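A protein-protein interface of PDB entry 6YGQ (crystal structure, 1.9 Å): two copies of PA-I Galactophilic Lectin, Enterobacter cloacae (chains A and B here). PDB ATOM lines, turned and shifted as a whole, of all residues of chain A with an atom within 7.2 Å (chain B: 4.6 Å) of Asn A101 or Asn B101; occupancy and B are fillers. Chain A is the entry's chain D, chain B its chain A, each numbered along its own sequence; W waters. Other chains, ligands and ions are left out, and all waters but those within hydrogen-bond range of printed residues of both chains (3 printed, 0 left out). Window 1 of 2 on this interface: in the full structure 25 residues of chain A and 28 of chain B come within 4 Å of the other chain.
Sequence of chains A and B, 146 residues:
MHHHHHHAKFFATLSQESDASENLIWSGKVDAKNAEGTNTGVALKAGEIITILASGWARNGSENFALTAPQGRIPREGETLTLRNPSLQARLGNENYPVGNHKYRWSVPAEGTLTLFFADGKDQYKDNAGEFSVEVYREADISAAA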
ATOM      1  N   ILE A  52      34.374   5.531   2.299  1.00  0.00           N
ATOM      2  CA  ILE A  52      33.010   5.123   1.987  1.00  0.00           C
ATOM      3  C   ILE A  52      32.107   5.641   3.097  1.00  0.00           C
ATOM      4  O   ILE A  52      32.392   5.427   4.281  1.00  0.00           O
ATOM      5  CB  ILE A  52      32.894   3.594   1.853  1.00  0.00           C
ATOM      6  CG1 ILE A  52      33.900   3.065   0.824  1.00  0.00           C
ATOM      7  CG2 ILE A  52      31.480   3.196   1.462  1.00  0.00           C
ATOM      8  CD1 ILE A  52      34.004   1.545   0.777  1.00  0.00           C
ATOM      9  N   LEU A  53      31.027   6.322   2.718  1.00  0.00           N
ATOM     10  CA  LEU A  53      30.077   6.886   3.668  1.00  0.00           C
ATOM     11  C   LEU A  53      28.672   6.449   3.285  1.00  0.00           C
ATOM     12  O   LEU A  53      28.343   6.371   2.097  1.00  0.00           O
ATOM     13  CB  LEU A  53      30.169   8.414   3.699  1.00  0.00           C
ATOM     14  CG  LEU A  53      31.574   8.994   3.883  1.00  0.00           C
ATOM     15  CD1 LEU A  53      31.541  10.518   3.804  1.00  0.00           C
ATOM     16  CD2 LEU A  53      32.190   8.536   5.201  1.00  0.00           C
ATOM     17  N   ALA A  54      27.839   6.173   4.290  1.00  0.00           N
ATOM     18  CA  ALA A  54      26.537   5.580   4.028  1.00  0.00           C
ATOM     19  C   ALA A  54      25.511   6.046   5.048  1.00  0.00           C
ATOM     20  O   ALA A  54      25.846   6.383   6.186  1.00  0.00           O
ATOM     21  CB  ALA A  54      26.612   4.046   4.051  1.00  0.00           C
ATOM     22  N   SER A  55      24.249   6.037   4.626  1.00  0.00           N
ATOM     23  CA  SER A  55      23.135   6.372   5.501  1.00  0.00           C
ATOM     24  C   SER A  55      21.871   5.748   4.929  1.00  0.00           C
ATOM     25  O   SER A  55      21.829   5.345   3.764  1.00  0.00           O
ATOM     26  CB  SER A  55      22.964   7.886   5.634  1.00  0.00           C
ATOM     27  OG  SER A  55      22.690   8.460   4.368  1.00  0.00           O
ATOM     28  N   GLY A  56      20.841   5.680   5.761  1.00  0.00           N
ATOM     29  CA  GLY A  56      19.532   5.235   5.327  1.00  0.00           C
ATOM     30  C   GLY A  56      18.950   4.181   6.250  1.00  0.00           C
ATOM     31  O   GLY A  56      19.582   3.699   7.182  1.00  0.00           O
ATOM     32  N   ALA A  69      20.101  -0.040   9.865  1.00  0.00           N
ATOM     33  CA  ALA A  69      20.867   1.072   9.321  1.00  0.00           C
ATOM     34  C   ALA A  69      22.137   0.479   8.712  1.00  0.00           C
ATOM     35  O   ALA A  69      22.369  -0.737   8.836  1.00  0.00           O
ATOM     36  CB  ALA A  69      21.205   2.092  10.397  1.00  0.00           C
ATOM     37  N   PRO A  70      22.980   1.271   8.054  1.00  0.00           N
ATOM     38  CA  PRO A  70      24.244   0.703   7.565  1.00  0.00           C
ATOM     39  C   PRO A  70      25.039   0.038   8.674  1.00  0.00           C
ATOM     40  O   PRO A  70      25.733  -0.955   8.423  1.00  0.00           O
ATOM     41  CB  PRO A  70      24.963   1.918   6.965  1.00  0.00           C
ATOM     42  CG  PRO A  70      23.841   2.846   6.555  1.00  0.00           C
ATOM     43  CD  PRO A  70      22.798   2.676   7.641  1.00  0.00           C
ATOM     44  N   GLN A  71      24.916   0.537   9.908  1.00  0.00           N
ATOM     45  CA  GLN A  71      25.591  -0.001  11.082  1.00  0.00           C
ATOM     46  C   GLN A  71      24.913  -1.248  11.656  1.00  0.00           C
ATOM     47  O   GLN A  71      25.251  -1.654  12.774  1.00  0.00           O
ATOM     48  CB  GLN A  71      25.680   1.081  12.170  1.00  0.00           C
ATOM     49  CG  GLN A  71      24.322   1.626  12.628  1.00  0.00           C
ATOM     50  CD  GLN A  71      24.423   2.652  13.753  1.00  0.00           C
ATOM     51  OE1 GLN A  71      25.427   3.354  13.888  1.00  0.00           O
ATOM     52  NE2 GLN A  71      23.370   2.745  14.564  1.00  0.00           N
ATOM     53  N   GLY A  72      23.973  -1.857  10.942  1.00  0.00           N
ATOM     54  CA  GLY A  72      23.386  -3.118  11.353  1.00  0.00           C
ATOM     55  C   GLY A  72      21.980  -2.949  11.904  1.00  0.00           C
ATOM     56  O   GLY A  72      21.410  -1.857  11.927  1.00  0.00           O
ATOM     57  N   LEU A  83      26.203  -2.121  18.832  1.00  0.00           N
ATOM     58  CA  LEU A  83      26.241  -2.345  17.395  1.00  0.00           C
ATOM     59  C   LEU A  83      26.354  -3.841  17.127  1.00  0.00           C
ATOM     60  O   LEU A  83      27.128  -4.549  17.774  1.00  0.00           O
ATOM     61  CB  LEU A  83      27.419  -1.608  16.768  1.00  0.00           C
ATOM     62  CG  LEU A  83      27.312  -0.086  16.671  1.00  0.00           C
ATOM     63  CD1 LEU A  83      28.539   0.452  15.949  1.00  0.00           C
ATOM     64  CD2 LEU A  83      26.037   0.348  15.965  1.00  0.00           C
ATOM     65  N   PRO A  86      27.313  -5.387  10.838  1.00  0.00           N
ATOM     66  CA  PRO A  86      27.076  -4.286   9.891  1.00  0.00           C
ATOM     67  C   PRO A  86      26.259  -4.749   8.694  1.00  0.00           C
ATOM     68  O   PRO A  86      26.571  -5.757   8.056  1.00  0.00           O
ATOM     69  CB  PRO A  86      28.491  -3.854   9.483  1.00  0.00           C
ATOM     70  CG  PRO A  86      29.393  -4.384  10.558  1.00  0.00           C
ATOM     71  CD  PRO A  86      28.750  -5.651  11.035  1.00  0.00           C
ATOM     72  N   LEU A  88      25.688  -2.913   5.861  1.00  0.00           N
ATOM     73  CA  LEU A  88      26.378  -2.523   4.639  1.00  0.00           C
ATOM     74  C   LEU A  88      27.807  -3.049   4.686  1.00  0.00           C
ATOM     75  O   LEU A  88      28.537  -2.793   5.648  1.00  0.00           O
ATOM     76  CB  LEU A  88      26.383  -1.004   4.457  1.00  0.00           C
ATOM     77  CG  LEU A  88      27.127  -0.523   3.208  1.00  0.00           C
ATOM     78  CD1 LEU A  88      26.435  -1.008   1.938  1.00  0.00           C
ATOM     79  CD2 LEU A  88      27.258   0.993   3.190  1.00  0.00           C
ATOM     80  N   VAL A  99      31.479  -2.197   6.181  1.00  0.00           N
ATOM     81  CA  VAL A  99      31.488  -0.762   5.959  1.00  0.00           C
ATOM     82  C   VAL A  99      30.723  -0.040   7.059  1.00  0.00           C
ATOM     83  O   VAL A  99      31.245   0.876   7.695  1.00  0.00           O
ATOM     84  CB  VAL A  99      30.916  -0.414   4.566  1.00  0.00           C
ATOM     85  CG1 VAL A  99      30.736   1.091   4.422  1.00  0.00           C
ATOM     86  CG2 VAL A  99      31.823  -0.964   3.469  1.00  0.00           C
ATOM     87  N   GLY A 100      29.491  -0.465   7.319  1.00  0.00           N
ATOM     88  CA  GLY A 100      28.689   0.251   8.283  1.00  0.00           C
ATOM     89  C   GLY A 100      28.382   1.655   7.787  1.00  0.00           C
ATOM     90  O   GLY A 100      28.237   1.905   6.586  1.00  0.00           O
ATOM     91  N   ASN A 101      28.281   2.586   8.740  1.00  0.00           N
ATOM     92  CA  ASN A 101      28.018   3.975   8.398  1.00  0.00           C
ATOM     93  C   ASN A 101      29.183   4.615   7.654  1.00  0.00           C
ATOM     94  O   ASN A 101      28.980   5.606   6.943  1.00  0.00           O
ATOM     95  CB  ASN A 101      27.756   4.817   9.653  1.00  0.00           C
ATOM     96  CG  ASN A 101      26.542   4.364  10.436  1.00  0.00           C
ATOM     97  OD1 ASN A 101      25.666   3.670   9.921  1.00  0.00           O
ATOM     98  ND2 ASN A 101      26.477   4.780  11.698  1.00  0.00           N
ATOM     99  N   HIS A 102      30.396   4.099   7.829  1.00  0.00           N
ATOM    100  CA  HIS A 102      31.561   4.766   7.272  1.00  0.00           C
ATOM    101  C   HIS A 102      32.774   3.854   7.370  1.00  0.00           C
ATOM    102  O   HIS A 102      32.970   3.173   8.379  1.00  0.00           O
ATOM    103  CB  HIS A 102      31.839   6.088   8.006  1.00  0.00           C
ATOM    104  CG  HIS A 102      32.003   5.935   9.489  1.00  0.00           C
ATOM    105  ND1 HIS A 102      33.185   5.527  10.070  1.00  0.00           N
ATOM    106  CD2 HIS A 102      31.133   6.132  10.507  1.00  0.00           C
ATOM    107  CE1 HIS A 102      33.037   5.483  11.381  1.00  0.00           C
ATOM    108  NE2 HIS A 102      31.800   5.843  11.674  1.00  0.00           N
ATOM    109  N   LYS A 103      33.572   3.847   6.305  1.00  0.00           N
ATOM    110  CA  LYS A 103      34.896   3.225   6.289  1.00  0.00           C
ATOM    111  C   LYS A 103      35.847   4.317   5.805  1.00  0.00           C
ATOM    112  O   LYS A 103      35.927   4.589   4.603  1.00  0.00           O
ATOM    113  CB  LYS A 103      34.936   1.993   5.395  1.00  0.00           C
ATOM    114  CG  LYS A 103      36.091   1.051   5.707  1.00  0.00           C
ATOM    115  CD  LYS A 103      35.965  -0.271   4.960  1.00  0.00           C
ATOM    116  CE  LYS A 103      36.920  -1.317   5.517  1.00  0.00           C
ATOM    117  NZ  LYS A 103      36.438  -1.885   6.808  1.00  0.00           N
ATOM    118  N   SER A 133      21.974   4.997   0.901  1.00  0.00           N
ATOM    119  CA  SER A 133      22.679   5.950   0.053  1.00  0.00           C
ATOM    120  C   SER A 133      24.154   5.915   0.428  1.00  0.00           C
ATOM    121  O   SER A 133      24.498   6.015   1.610  1.00  0.00           O
ATOM    122  CB  SER A 133      22.117   7.359   0.232  1.00  0.00           C
ATOM    123  OG  SER A 133      20.717   7.382   0.021  1.00  0.00           O
ATOM    124  N   ILE B  52      33.812  14.438  10.644  1.00  0.00           N
ATOM    125  CA  ILE B  52      33.219  13.817  11.822  1.00  0.00           C
ATOM    126  C   ILE B  52      32.506  12.548  11.374  1.00  0.00           C
ATOM    127  O   ILE B  52      31.759  12.567  10.389  1.00  0.00           O
ATOM    128  CB  ILE B  52      32.247  14.770  12.540  1.00  0.00           C
ATOM    129  CG1 ILE B  52      32.928  16.109  12.842  1.00  0.00           C
ATOM    130  CG2 ILE B  52      31.741  14.133  13.828  1.00  0.00           C
ATOM    131  CD1 ILE B  52      31.956  17.254  13.054  1.00  0.00           C
ATOM    132  N   LEU B  53      32.747  11.449  12.091  1.00  0.00           N
ATOM    133  CA  LEU B  53      32.146  10.155  11.800  1.00  0.00           C
ATOM    134  C   LEU B  53      31.537   9.581  13.070  1.00  0.00           C
ATOM    135  O   LEU B  53      32.131   9.689  14.146  1.00  0.00           O
ATOM    136  CB  LEU B  53      33.181   9.175  11.246  1.00  0.00           C
ATOM    137  CG  LEU B  53      34.026   9.680  10.078  1.00  0.00           C
ATOM    138  CD1 LEU B  53      35.168   8.713   9.805  1.00  0.00           C
ATOM    139  CD2 LEU B  53      33.161   9.868   8.846  1.00  0.00           C
ATOM    140  N   ALA B  54      30.373   8.943  12.945  1.00  0.00           N
ATOM    141  CA  ALA B  54      29.664   8.489  14.132  1.00  0.00           C
ATOM    142  C   ALA B  54      28.909   7.195  13.874  1.00  0.00           C
ATOM    143  O   ALA B  54      28.575   6.851  12.738  1.00  0.00           O
ATOM    144  CB  ALA B  54      28.689   9.564  14.635  1.00  0.00           C
ATOM    145  N   SER B  55      28.639   6.484  14.968  1.00  0.00           N
ATOM    146  CA  SER B  55      27.869   5.249  14.951  1.00  0.00           C
ATOM    147  C   SER B  55      27.296   5.038  16.346  1.00  0.00           C
ATOM    148  O   SER B  55      27.755   5.640  17.320  1.00  0.00           O
ATOM    149  CB  SER B  55      28.733   4.054  14.537  1.00  0.00           C
ATOM    150  OG  SER B  55      29.760   3.815  15.487  1.00  0.00           O
ATOM    151  N   PRO B  70      22.890   7.892  14.775  1.00  0.00           N
ATOM    152  CA  PRO B  70      23.352   9.266  14.487  1.00  0.00           C
ATOM    153  C   PRO B  70      22.511   9.943  13.416  1.00  0.00           C
ATOM    154  O   PRO B  70      22.222  11.142  13.512  1.00  0.00           O
ATOM    155  CB  PRO B  70      24.809   9.064  14.053  1.00  0.00           C
ATOM    156  CG  PRO B  70      25.234   7.822  14.800  1.00  0.00           C
ATOM    157  CD  PRO B  70      24.012   6.932  14.812  1.00  0.00           C
ATOM    158  N   GLN B  71      22.075   9.184  12.413  1.00  0.00           N
ATOM    159  CA  GLN B  71      21.225   9.690  11.341  1.00  0.00           C
ATOM    160  C   GLN B  71      19.780   9.959  11.780  1.00  0.00           C
ATOM    161  O   GLN B  71      18.947  10.211  10.902  1.00  0.00           O
ATOM    162  CB  GLN B  71      21.232   8.699  10.174  1.00  0.00           C
ATOM    163  CG  GLN B  71      20.811   7.287  10.556  1.00  0.00           C
ATOM    164  CD  GLN B  71      20.833   6.332   9.378  1.00  0.00           C
ATOM    165  OE1 GLN B  71      21.628   6.486   8.450  1.00  0.00           O
ATOM    166  NE2 GLN B  71      19.953   5.339   9.408  1.00  0.00           N
ATOM    167  N   VAL B  99      25.042  16.757  12.007  1.00  0.00           N
ATOM    168  CA  VAL B  99      26.176  15.881  11.712  1.00  0.00           C
ATOM    169  C   VAL B  99      25.679  14.546  11.161  1.00  0.00           C
ATOM    170  O   VAL B  99      26.096  14.124  10.077  1.00  0.00           O
ATOM    171  CB  VAL B  99      27.047  15.662  12.962  1.00  0.00           C
ATOM    172  CG1 VAL B  99      28.117  14.598  12.695  1.00  0.00           C
ATOM    173  CG2 VAL B  99      27.688  16.973  13.392  1.00  0.00           C
ATOM    174  N   GLY B 100      24.796  13.872  11.897  1.00  0.00           N
ATOM    175  CA  GLY B 100      24.335  12.575  11.434  1.00  0.00           C
ATOM    176  C   GLY B 100      25.432  11.529  11.543  1.00  0.00           C
ATOM    177  O   GLY B 100      26.302  11.588  12.419  1.00  0.00           O
ATOM    178  N   ASN B 101      25.386  10.551  10.629  1.00  0.00           N
ATOM    179  CA  ASN B 101      26.407   9.511  10.605  1.00  0.00           C
ATOM    180  C   ASN B 101      27.778  10.077  10.259  1.00  0.00           C
ATOM    181  O   ASN B 101      28.803   9.517  10.667  1.00  0.00           O
ATOM    182  CB  ASN B 101      26.074   8.432   9.573  1.00  0.00           C
ATOM    183  CG  ASN B 101      24.837   7.637   9.920  1.00  0.00           C
ATOM    184  OD1 ASN B 101      24.314   7.718  11.031  1.00  0.00           O
ATOM    185  ND2 ASN B 101      24.360   6.852   8.958  1.00  0.00           N
ATOM    186  N   HIS B 102      27.823  11.141   9.465  1.00  0.00           N
ATOM    187  CA  HIS B 102      29.101  11.639   8.986  1.00  0.00           C
ATOM    188  C   HIS B 102      28.936  13.042   8.429  1.00  0.00           C
ATOM    189  O   HIS B 102      27.935  13.348   7.776  1.00  0.00           O
ATOM    190  CB  HIS B 102      29.690  10.714   7.910  1.00  0.00           C
ATOM    191  CG  HIS B 102      28.704  10.291   6.863  1.00  0.00           C
ATOM    192  ND1 HIS B 102      28.369  11.089   5.790  1.00  0.00           N
ATOM    193  CD2 HIS B 102      27.995   9.147   6.717  1.00  0.00           C
ATOM    194  CE1 HIS B 102      27.490  10.458   5.033  1.00  0.00           C
ATOM    195  NE2 HIS B 102      27.243   9.279   5.574  1.00  0.00           N
HETATM  196  O   HOH W   1      31.960   5.847  14.804  1.00  0.00           O
HETATM  197  O   HOH W   2      25.318   8.809   2.979  1.00  0.00           O
HETATM  198  O   HOH W   3      23.277   4.876  11.198  1.00  0.00           O
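Of the printed residues of chain B, Ala A54 touches Asn B101 and His B102. Of the printed residues of chain B, Ser A55 touches Gln B71 (3.3 Å) and Asn B101 (3.7 Å). Leu A88 touches none of the printed residues of chain B. Gly A100 touches none of the printed residues of chain B. Of chain B, only Ala B54, Ser B55, Asn B101 and His B102 come within 4 Å of Asn A101. Printed residues of chain B within 4 Å of His A102: Leu B53 (3.6 Å) and Ala B54 (3.5 Å). Asn B101 touches three residues of chain A. Of the printed residues of chain A, His B102 touches Leu A53 (3.6 Å), Ala A54 (3.3 Å) and Asn A101 (3.7 Å). The nearest residue of chain A that does not touch Asn B101 is His A102 (4.1 Å).
Ala A54 touches His B102, and with the chains exchanged His A102 touches Ala B54. Ser A55 touches Gln B71, and with the chains exchanged Gln A71 touches Ser B55. Ser A55 touches Asn B101, and with the chains exchanged Asn A101 touches Ser B55. Asn A101 touches His B102, but with the chains exchanged His A102 does not touch Asn B101 (4.1 Å). Positions printed for both chains: 52, 53, 54, 55, 70, 71, 99, 100, 101 and 102. Of the 16 pairs that touch across the chains among the printed residues, 11 have their exchanged pair printed and touching as well.
Of the 10 printed residues of chain B, 7 touch a printed residue of chain A. Hydrophobic or aromatic side chains of chain B within 4 Å of the printed part of chain A: Leu B53, Pro B70 and His B102. Of the 18 printed residues of chain A, 9 touch a printed residue of chain B. Hydrophobic or aromatic side chains of chain A within 4 Å of the printed part of chain B: Leu A53, Ala A69, Leu A83 and His A102. Among the printed residues, no Asp or Glu carboxylate lies within 4 Å of a Lys or Arg side-chain nitrogen of the other chain.
O of Asn B101 is in hydrogen-bond range of N of Ala B54. The side-chain amide oxygen of Gln A71 sits at hydrogen-bond distance from the side-chain amide nitrogen of Asn A101 (2.8 Å). OE1 of Gln B71 lies within hydrogen-bond range of ND2 of Asn B101. N of Ala A54 lies within hydrogen-bond range of O of Asn A101, 2.9 Å away. The backbone carbonyl oxygen (O) of Ser A55 sits at hydrogen-bond distance from the backbone NH (N) of Ser A133 (2.9 Å).
Water W3 bridges OD1 of Asn A101 and OD1 of Asn B101. Water W2 lies within hydrogen-bond range of the side-chain hydroxyl of Ser A55, the backbone carbonyl oxygen of Ser A133 and a ring nitrogen (NE2) of His B102. Water W1 bridges OG of Ser B55 and NE2 of His A102.
The side-chain amide nitrogen of Asn A101 lies within hydrogen-bond range of the backbone carbonyl oxygen of Ala B54 (3.1 Å). The backbone carbonyl oxygen of Ala A54 sits at hydrogen-bond distance from a ring nitrogen (NE2) of His B102, 3.3 Å away. The side-chain amide nitrogen (NE2) of Gln B71 sits at hydrogen-bond distance from the backbone carbonyl oxygen (O) of Gly A56, at 2.8 Å. The side-chain amide nitrogen (ND2) of Asn B101 is in hydrogen-bond range of the backbone carbonyl oxygen (O) of Ala A54 (3.2 Å).
Among the printed residues, merely in contact across the chains: Leu A53 with His B102 (3.6 Å), Ser A55 with Gln B71 (3.3 Å), Ser A55 with Asn B101 (3.7 Å), Ala A69 with Gln B71 (3.6 Å), Gln A71 with Ser B55 (3.3 Å), Gln A71 with Pro B70 (3.96 Å), Leu A83 with Ser B55 (3.6 Å), Asn A101 with Ser B55 (3.6 Å), Asn A101 with Asn B101 (3.6 Å), Asn A101 with His B102 (3.7 Å), His A102 with Leu B53 (3.6 Å) and His A102 with Ala B54 (3.5 Å).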
